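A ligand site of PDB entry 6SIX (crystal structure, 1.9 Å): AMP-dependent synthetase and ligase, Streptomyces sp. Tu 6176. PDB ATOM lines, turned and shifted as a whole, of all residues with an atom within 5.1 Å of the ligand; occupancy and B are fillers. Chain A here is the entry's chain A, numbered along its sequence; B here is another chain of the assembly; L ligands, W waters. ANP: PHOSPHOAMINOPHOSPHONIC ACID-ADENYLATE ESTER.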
ATOM      1  N   LYS A  63       0.373  29.803 -10.288  1.00  0.00           N
ATOM      2  CA  LYS A  63      -0.540  30.659 -11.099  1.00  0.00           C
ATOM      3  C   LYS A  63       0.287  31.603 -11.969  1.00  0.00           C
ATOM      4  O   LYS A  63      -0.070  31.802 -13.126  1.00  0.00           O
ATOM      5  CB  LYS A  63      -1.424  31.524 -10.205  1.00  0.00           C
ATOM      6  CG  LYS A  63      -2.633  30.822  -9.601  1.00  0.00           C
ATOM      7  CD  LYS A  63      -3.735  31.820  -9.266  1.00  0.00           C
ATOM      8  CE  LYS A  63      -5.040  31.148  -8.887  1.00  0.00           C
ATOM      9  NZ  LYS A  63      -4.832  30.086  -7.882  1.00  0.00           N
ATOM     10  N   GLU A  87     -10.708  31.675 -20.108  1.00  0.00           N
ATOM     11  CA  GLU A  87      -9.802  32.492 -19.273  1.00  0.00           C
ATOM     12  C   GLU A  87     -10.405  32.544 -17.883  1.00  0.00           C
ATOM     13  O   GLU A  87     -11.611  32.508 -17.772  1.00  0.00           O
ATOM     14  CB  GLU A  87      -9.607  33.877 -19.857  1.00  0.00           C
ATOM     15  CG  GLU A  87      -8.872  33.833 -21.169  1.00  0.00           C
ATOM     16  CD  GLU A  87      -8.489  35.185 -21.762  1.00  0.00           C
ATOM     17  OE1 GLU A  87      -8.814  36.231 -21.142  1.00  0.00           O
ATOM     18  OE2 GLU A  87      -7.881  35.181 -22.830  1.00  0.00           O
ATOM     19  N   SER A  88      -9.561  32.640 -16.871  1.00  0.00           N
ATOM     20  CA  SER A  88      -9.974  32.586 -15.453  1.00  0.00           C
ATOM     21  C   SER A  88     -10.619  33.921 -15.104  1.00  0.00           C
ATOM     22  O   SER A  88     -10.281  34.937 -15.749  1.00  0.00           O
ATOM     23  CB  SER A  88      -8.803  32.252 -14.543  1.00  0.00           C
ATOM     24  OG  SER A  88      -8.382  30.912 -14.755  1.00  0.00           O
ATOM     25  N   SER A  89     -11.486  33.905 -14.091  1.00  0.00           N
ATOM     26  CA  SER A  89     -12.028  35.099 -13.389  1.00  0.00           C
ATOM     27  C   SER A  89     -10.849  35.818 -12.692  1.00  0.00           C
ATOM     28  O   SER A  89      -9.681  35.372 -12.837  1.00  0.00           O
ATOM     29  CB  SER A  89     -13.134  34.698 -12.441  1.00  0.00           C
ATOM     30  OG  SER A  89     -12.600  34.059 -11.285  1.00  0.00           O
ATOM     31  N   GLY A  90     -11.127  36.911 -11.977  1.00  0.00           N
ATOM     32  CA  GLY A  90     -10.079  37.724 -11.325  1.00  0.00           C
ATOM     33  C   GLY A  90      -9.485  38.754 -12.266  1.00  0.00           C
ATOM     34  O   GLY A  90     -10.232  39.238 -13.167  1.00  0.00           O
ATOM     35  N   VAL A 134     -15.027  32.452 -18.950  1.00  0.00           N
ATOM     36  CA  VAL A 134     -14.876  31.480 -17.835  1.00  0.00           C
ATOM     37  C   VAL A 134     -15.563  30.153 -18.210  1.00  0.00           C
ATOM     38  O   VAL A 134     -16.466  30.147 -19.073  1.00  0.00           O
ATOM     39  CB  VAL A 134     -15.426  32.015 -16.500  1.00  0.00           C
ATOM     40  CG1 VAL A 134     -14.621  33.208 -16.012  1.00  0.00           C
ATOM     41  CG2 VAL A 134     -16.906  32.356 -16.575  1.00  0.00           C
ATOM     42  N   ALA A 212     -20.738  26.685  -5.711  1.00  0.00           N
ATOM     43  CA  ALA A 212     -19.268  26.705  -5.637  1.00  0.00           C
ATOM     44  C   ALA A 212     -18.815  28.165  -5.693  1.00  0.00           C
ATOM     45  O   ALA A 212     -19.680  29.041  -5.729  1.00  0.00           O
ATOM     46  CB  ALA A 212     -18.665  25.946  -6.785  1.00  0.00           C
ATOM     47  N   ALA A 213     -17.499  28.371  -5.793  1.00  0.00           N
ATOM     48  CA  ALA A 213     -16.830  29.621  -6.222  1.00  0.00           C
ATOM     49  C   ALA A 213     -16.607  30.539  -5.023  1.00  0.00           C
ATOM     50  O   ALA A 213     -15.858  31.524  -5.185  1.00  0.00           O
ATOM     51  CB  ALA A 213     -17.623  30.307  -7.312  1.00  0.00           C
ATOM     52  N   GLU A 214     -17.205  30.250  -3.863  1.00  0.00           N
ATOM     53  CA  GLU A 214     -17.025  31.042  -2.609  1.00  0.00           C
ATOM     54  C   GLU A 214     -16.716  30.094  -1.454  1.00  0.00           C
ATOM     55  O   GLU A 214     -17.327  29.029  -1.347  1.00  0.00           O
ATOM     56  CB  GLU A 214     -18.285  31.775  -2.180  1.00  0.00           C
ATOM     57  CG  GLU A 214     -18.572  33.040  -2.925  1.00  0.00           C
ATOM     58  CD  GLU A 214     -19.856  33.726  -2.459  1.00  0.00           C
ATOM     59  OE1 GLU A 214     -20.725  33.999  -3.323  1.00  0.00           O
ATOM     60  OE2 GLU A 214     -19.968  34.000  -1.225  1.00  0.00           O
ATOM     61  N   PRO A 215     -15.862  30.529  -0.512  1.00  0.00           N
ATOM     62  CA  PRO A 215     -15.766  29.851   0.788  1.00  0.00           C
ATOM     63  C   PRO A 215     -17.142  29.871   1.462  1.00  0.00           C
ATOM     64  O   PRO A 215     -17.798  30.904   1.471  1.00  0.00           O
ATOM     65  CB  PRO A 215     -14.761  30.688   1.589  1.00  0.00           C
ATOM     66  CG  PRO A 215     -14.003  31.470   0.520  1.00  0.00           C
ATOM     67  CD  PRO A 215     -14.974  31.685  -0.612  1.00  0.00           C
ATOM     68  N   LEU A 216     -17.596  28.715   1.916  1.00  0.00           N
ATOM     69  CA  LEU A 216     -18.987  28.532   2.373  1.00  0.00           C
ATOM     70  C   LEU A 216     -18.971  27.778   3.697  1.00  0.00           C
ATOM     71  O   LEU A 216     -18.634  26.604   3.675  1.00  0.00           O
ATOM     72  CB  LEU A 216     -19.778  27.801   1.287  1.00  0.00           C
ATOM     73  CG  LEU A 216     -21.262  27.575   1.567  1.00  0.00           C
ATOM     74  CD1 LEU A 216     -21.967  28.896   1.822  1.00  0.00           C
ATOM     75  CD2 LEU A 216     -21.914  26.814   0.428  1.00  0.00           C
ATOM     76  N   GLU A 235     -22.476  21.537  -2.539  1.00  0.00           N
ATOM     77  CA  GLU A 235     -21.238  22.302  -2.809  1.00  0.00           C
ATOM     78  C   GLU A 235     -20.282  21.491  -3.658  1.00  0.00           C
ATOM     79  O   GLU A 235     -20.206  20.255  -3.486  1.00  0.00           O
ATOM     80  CB  GLU A 235     -20.565  22.619  -1.480  1.00  0.00           C
ATOM     81  CG  GLU A 235     -19.519  23.698  -1.592  1.00  0.00           C
ATOM     82  CD  GLU A 235     -18.850  24.038  -0.273  1.00  0.00           C
ATOM     83  OE1 GLU A 235     -19.192  23.407   0.763  1.00  0.00           O
ATOM     84  OE2 GLU A 235     -17.987  24.929  -0.280  1.00  0.00           O
ATOM     85  N   GLU A 236     -19.536  22.175  -4.519  1.00  0.00           N
ATOM     86  CA  GLU A 236     -18.309  21.611  -5.136  1.00  0.00           C
ATOM     87  C   GLU A 236     -17.196  22.668  -5.064  1.00  0.00           C
ATOM     88  O   GLU A 236     -17.469  23.827  -4.759  1.00  0.00           O
ATOM     89  CB  GLU A 236     -18.579  21.113  -6.547  1.00  0.00           C
ATOM     90  CG  GLU A 236     -18.795  22.219  -7.582  1.00  0.00           C
ATOM     91  CD  GLU A 236     -18.602  21.676  -8.988  1.00  0.00           C
ATOM     92  OE1 GLU A 236     -19.303  20.700  -9.334  1.00  0.00           O
ATOM     93  OE2 GLU A 236     -17.710  22.178  -9.716  1.00  0.00           O
ATOM     94  N   TYR A 237     -15.972  22.223  -5.297  1.00  0.00           N
ATOM     95  CA  TYR A 237     -14.729  23.027  -5.285  1.00  0.00           C
ATOM     96  C   TYR A 237     -14.045  22.800  -6.625  1.00  0.00           C
ATOM     97  O   TYR A 237     -13.889  21.610  -7.018  1.00  0.00           O
ATOM     98  CB  TYR A 237     -13.899  22.615  -4.077  1.00  0.00           C
ATOM     99  CG  TYR A 237     -12.497  23.185  -4.002  1.00  0.00           C
ATOM    100  CD1 TYR A 237     -12.218  24.482  -4.413  1.00  0.00           C
ATOM    101  CD2 TYR A 237     -11.464  22.435  -3.472  1.00  0.00           C
ATOM    102  CE1 TYR A 237     -10.941  25.008  -4.316  1.00  0.00           C
ATOM    103  CE2 TYR A 237     -10.190  22.951  -3.366  1.00  0.00           C
ATOM    104  CZ  TYR A 237      -9.922  24.241  -3.787  1.00  0.00           C
ATOM    105  OH  TYR A 237      -8.659  24.749  -3.692  1.00  0.00           O
ATOM    106  N   GLY A 238     -13.719  23.883  -7.329  1.00  0.00           N
ATOM    107  CA  GLY A 238     -13.157  23.838  -8.681  1.00  0.00           C
ATOM    108  C   GLY A 238     -12.481  25.126  -9.070  1.00  0.00           C
ATOM    109  O   GLY A 238     -12.415  26.043  -8.230  1.00  0.00           O
ATOM    110  N   SER A 239     -11.993  25.186 -10.303  1.00  0.00           N
ATOM    111  CA  SER A 239     -11.386  26.387 -10.938  1.00  0.00           C
ATOM    112  C   SER A 239     -11.466  26.198 -12.450  1.00  0.00           C
ATOM    113  O   SER A 239     -11.640  25.033 -12.882  1.00  0.00           O
ATOM    114  CB  SER A 239      -9.957  26.585 -10.460  1.00  0.00           C
ATOM    115  OG  SER A 239      -9.070  25.658 -11.086  1.00  0.00           O
ATOM    116  N   THR A 240     -11.352  27.280 -13.227  1.00  0.00           N
ATOM    117  CA  THR A 240     -11.356  27.247 -14.711  1.00  0.00           C
ATOM    118  C   THR A 240     -10.224  26.341 -15.201  1.00  0.00           C
ATOM    119  O   THR A 240     -10.426  25.605 -16.194  1.00  0.00           O
ATOM    120  CB  THR A 240     -11.295  28.682 -15.261  1.00  0.00           C
ATOM    121  OG1 THR A 240     -12.493  29.329 -14.831  1.00  0.00           O
ATOM    122  CG2 THR A 240     -11.161  28.752 -16.764  1.00  0.00           C
ATOM    123  N   GLU A 241      -9.075  26.349 -14.525  1.00  0.00           N
ATOM    124  CA  GLU A 241      -7.873  25.654 -15.046  1.00  0.00           C
ATOM    125  C   GLU A 241      -7.877  24.170 -14.634  1.00  0.00           C
ATOM    126  O   GLU A 241      -7.121  23.428 -15.282  1.00  0.00           O
ATOM    127  CB  GLU A 241      -6.593  26.393 -14.643  1.00  0.00           C
ATOM    128  CG  GLU A 241      -6.467  26.686 -13.175  1.00  0.00           C
ATOM    129  CD  GLU A 241      -6.944  28.060 -12.715  1.00  0.00           C
ATOM    130  OE1 GLU A 241      -6.443  28.509 -11.652  1.00  0.00           O
ATOM    131  OE2 GLU A 241      -7.811  28.654 -13.390  1.00  0.00           O
ATOM    132  N   MET A 254     -17.115  17.773   1.464  1.00  0.00           N
ATOM    133  CA  MET A 254     -16.586  17.716   0.090  1.00  0.00           C
ATOM    134  C   MET A 254     -15.479  16.665   0.035  1.00  0.00           C
ATOM    135  O   MET A 254     -14.572  16.732   0.880  1.00  0.00           O
ATOM    136  CB  MET A 254     -16.044  19.069  -0.385  1.00  0.00           C
ATOM    137  CG  MET A 254     -17.153  20.074  -0.702  1.00  0.00           C
ATOM    138  SD  MET A 254     -16.527  21.517  -1.610  1.00  0.00           S
ATOM    139  CE  MET A 254     -15.463  22.261  -0.368  1.00  0.00           C
ATOM    140  N   TYR A 296       0.029  21.732  -9.800  1.00  0.00           N
ATOM    141  CA  TYR A 296      -0.465  23.124  -9.951  1.00  0.00           C
ATOM    142  C   TYR A 296      -1.004  23.583  -8.587  1.00  0.00           C
ATOM    143  O   TYR A 296      -1.903  22.925  -8.035  1.00  0.00           O
ATOM    144  CB  TYR A 296      -1.502  23.189 -11.071  1.00  0.00           C
ATOM    145  CG  TYR A 296      -2.200  24.521 -11.125  1.00  0.00           C
ATOM    146  CD1 TYR A 296      -1.496  25.677 -11.446  1.00  0.00           C
ATOM    147  CD2 TYR A 296      -3.537  24.629 -10.808  1.00  0.00           C
ATOM    148  CE1 TYR A 296      -2.126  26.909 -11.459  1.00  0.00           C
ATOM    149  CE2 TYR A 296      -4.187  25.857 -10.853  1.00  0.00           C
ATOM    150  CZ  TYR A 296      -3.477  26.991 -11.183  1.00  0.00           C
ATOM    151  OH  TYR A 296      -4.112  28.196 -11.227  1.00  0.00           O
ATOM    152  N   LEU A 298      -3.174  25.913  -6.665  1.00  0.00           N
ATOM    153  CA  LEU A 298      -4.342  26.816  -6.678  1.00  0.00           C
ATOM    154  C   LEU A 298      -4.144  27.943  -5.665  1.00  0.00           C
ATOM    155  O   LEU A 298      -4.901  28.929  -5.722  1.00  0.00           O
ATOM    156  CB  LEU A 298      -5.610  26.034  -6.310  1.00  0.00           C
ATOM    157  CG  LEU A 298      -6.337  25.342  -7.462  1.00  0.00           C
ATOM    158  CD1 LEU A 298      -7.434  24.452  -6.896  1.00  0.00           C
ATOM    159  CD2 LEU A 298      -6.948  26.362  -8.421  1.00  0.00           C
ATOM    160  N   ASP A 300      -5.075  28.038  -2.689  1.00  0.00           N
ATOM    161  CA  ASP A 300      -6.184  28.078  -1.709  1.00  0.00           C
ATOM    162  C   ASP A 300      -5.716  27.407  -0.418  1.00  0.00           C
ATOM    163  O   ASP A 300      -5.060  26.357  -0.509  1.00  0.00           O
ATOM    164  CB  ASP A 300      -7.460  27.383  -2.191  1.00  0.00           C
ATOM    165  CG  ASP A 300      -8.103  28.029  -3.403  1.00  0.00           C
ATOM    166  OD1 ASP A 300      -8.104  29.295  -3.490  1.00  0.00           O
ATOM    167  OD2 ASP A 300      -8.582  27.270  -4.282  1.00  0.00           O
ATOM    168  N   VAL A 320     -12.234  24.185   2.422  1.00  0.00           N
ATOM    169  CA  VAL A 320     -11.568  25.313   1.718  1.00  0.00           C
ATOM    170  C   VAL A 320     -11.811  26.578   2.540  1.00  0.00           C
ATOM    171  O   VAL A 320     -12.944  27.104   2.549  1.00  0.00           O
ATOM    172  CB  VAL A 320     -12.062  25.432   0.261  1.00  0.00           C
ATOM    173  CG1 VAL A 320     -11.254  26.449  -0.528  1.00  0.00           C
ATOM    174  CG2 VAL A 320     -12.051  24.081  -0.436  1.00  0.00           C
ATOM    175  N   LYS B 419     -15.587  37.997  -7.443  1.00  0.00           N
ATOM    176  CA  LYS B 419     -16.608  37.206  -6.711  1.00  0.00           C
ATOM    177  C   LYS B 419     -16.977  37.979  -5.439  1.00  0.00           C
ATOM    178  O   LYS B 419     -16.228  38.902  -5.071  1.00  0.00           O
ATOM    179  CB  LYS B 419     -16.072  35.818  -6.366  1.00  0.00           C
ATOM    180  CG  LYS B 419     -15.401  35.084  -7.530  1.00  0.00           C
ATOM    181  CD  LYS B 419     -15.568  33.570  -7.469  1.00  0.00           C
ATOM    182  CE  LYS B 419     -14.324  32.777  -7.850  1.00  0.00           C
ATOM    183  NZ  LYS B 419     -13.881  33.100  -9.229  1.00  0.00           N
HETATM  184  PG  ANP L   1      -8.783  31.801 -10.506  1.00  0.00           P
HETATM  185  O1G ANP L   1      -8.606  31.834  -9.002  1.00  0.00           O
HETATM  186  O2G ANP L   1      -8.171  33.097 -11.008  1.00  0.00           O
HETATM  187  O3G ANP L   1      -7.986  30.635 -11.063  1.00  0.00           O
HETATM  188  PB  ANP L   1     -11.030  30.663 -12.097  1.00  0.00           P
HETATM  189  O1B ANP L   1     -11.915  31.426 -13.049  1.00  0.00           O
HETATM  190  O2B ANP L   1     -10.006  29.722 -12.665  1.00  0.00           O
HETATM  191  N3B ANP L   1     -10.372  31.636 -10.932  1.00  0.00           N
HETATM  192  PA  ANP L   1     -13.330  30.097 -10.459  1.00  0.00           P
HETATM  193  O1A ANP L   1     -14.246  28.924 -10.282  1.00  0.00           O
HETATM  194  O2A ANP L   1     -13.948  31.357 -10.972  1.00  0.00           O
HETATM  195  O3A ANP L   1     -12.067  29.711 -11.370  1.00  0.00           O
HETATM  196  O5' ANP L   1     -12.569  30.403  -9.085  1.00  0.00           O
HETATM  197  C5' ANP L   1     -11.689  29.390  -8.541  1.00  0.00           C
HETATM  198  C4' ANP L   1     -11.428  29.684  -7.096  1.00  0.00           C
HETATM  199  O4' ANP L   1     -12.689  29.893  -6.400  1.00  0.00           O
HETATM  200  C3' ANP L   1     -10.760  28.565  -6.296  1.00  0.00           C
HETATM  201  O3' ANP L   1      -9.360  28.531  -6.517  1.00  0.00           O
HETATM  202  C2' ANP L   1     -11.120  29.013  -4.881  1.00  0.00           C
HETATM  203  O2' ANP L   1     -10.360  30.126  -4.458  1.00  0.00           O
HETATM  204  C1' ANP L   1     -12.575  29.434  -5.063  1.00  0.00           C
HETATM  205  N9  ANP L   1     -13.536  28.351  -4.816  1.00  0.00           N
HETATM  206  C8  ANP L   1     -14.225  27.569  -5.718  1.00  0.00           C
HETATM  207  N7  ANP L   1     -15.019  26.701  -5.145  1.00  0.00           N
HETATM  208  C5  ANP L   1     -14.874  26.922  -3.778  1.00  0.00           C
HETATM  209  C6  ANP L   1     -15.457  26.333  -2.644  1.00  0.00           C
HETATM  210  N6  ANP L   1     -16.359  25.359  -2.671  1.00  0.00           N
HETATM  211  N1  ANP L   1     -15.062  26.800  -1.427  1.00  0.00           N
HETATM  212  C2  ANP L   1     -14.157  27.793  -1.389  1.00  0.00           C
HETATM  213  N3  ANP L   1     -13.550  28.423  -2.390  1.00  0.00           N
HETATM  214  C4  ANP L   1     -13.961  27.937  -3.579  1.00  0.00           C
HETATM  215  O   HOH W   1     -19.139  27.391  -2.435  1.00  0.00           O
HETATM  216  O   HOH W   2      -7.705  29.594  -8.179  1.00  0.00           O
HETATM  217  O   HOH W   3     -11.618  30.298  -1.780  1.00  0.00           O
HETATM  218  O   HOH W   4     -15.680  27.340  -8.662  1.00  0.00           O
HETATM  219  O   HOH W   5     -16.194  26.163   0.977  1.00  0.00           O
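O2B of the ligand is in hydrogen-bond range of N of Thr 240 (2.8 Å).
The backbone NH (N) of Ala 213 is in hydrogen-bond range of a nitrogen (N7) of the ligand, at 3.1 Å.
OG of Ser 88 sits at hydrogen-bond distance from O2B of the ligand.
N of Ser 89 lies within hydrogen-bond range of O1B of the ligand, at 2.7 Å.
OE2 of Glu 235 lies within hydrogen-bond range of N6 of the ligand (2.9 Å).
OG of Ser 89 lies within hydrogen-bond range of O2A of the ligand (3.0 Å).
The side-chain carboxylate of Glu 241 lies close to an oxygen (O2B) of the ligand (2.5 Å).
O2' of the ligand is in hydrogen-bond range of OD1 of Asp 300, 2.6 Å away.
A nitrogen (N6) of the ligand sits at hydrogen-bond distance from the backbone carbonyl oxygen (O) of Glu 236 (2.8 Å).
The side-chain hydroxyl (OG1) of Thr 240 lies within hydrogen-bond range of an oxygen (O1B) of the ligand.
An oxygen (O2A) of the ligand is in salt-bridge range of the side-chain amino group of Lys 419 of chain B (2.5 Å).
Water W2 lies within hydrogen-bond range of an oxygen (O1G) of the ligand and the side-chain amino group (NZ) of Lys 63.
Water W5 lies within hydrogen-bond range of the side-chain carboxylate of Glu 235 (2.5 Å), a nitrogen (N1) of the ligand (2.7 Å) and the backbone NH of Leu 216 (3.1 Å).
Water W1 lies within hydrogen-bond range of the backbone carbonyl oxygen of Glu 214 (2.7 Å), a nitrogen (N6) of the ligand (3.5 Å) and the side-chain carboxylate of Glu 235 (3.5 Å).
The backbone carbonyl oxygen of Glu 214 lies close to a nitrogen (N1) of the ligand (3.2 Å).
Merely in contact with the ligand: Val 320, Pro 215, Ser 239, Gly 238, Lys 63, Tyr 237, Leu 298 and Met 254.
Hydrophobic or aromatic side chains within 4 Å of the ligand: Pro 215, Tyr 237, Met 254, Leu 298 and Val 320.
Of the 24 residues printed, 18 come within 4 Å of the ligand.
The nearest printed residue that does not touch the ligand is Ala 212 (4.1 Å).
NZ of Lys 419 of chain B sits at hydrogen-bond distance from OG of Ser 89, 2.6 Å away.
The side-chain hydroxyl of Ser 88 sits at hydrogen-bond distance from the side-chain carboxylate of Glu 241.
NZ of Lys 63 lies within hydrogen-bond range of O of Leu 298.
The side-chain carboxylate (OD2) of Asp 300 sits at hydrogen-bond distance from the side-chain hydroxyl (OH) of Tyr 237 (2.6 Å).
N of Tyr 237 sits close to SD of Met 254, 3.8 Å away.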
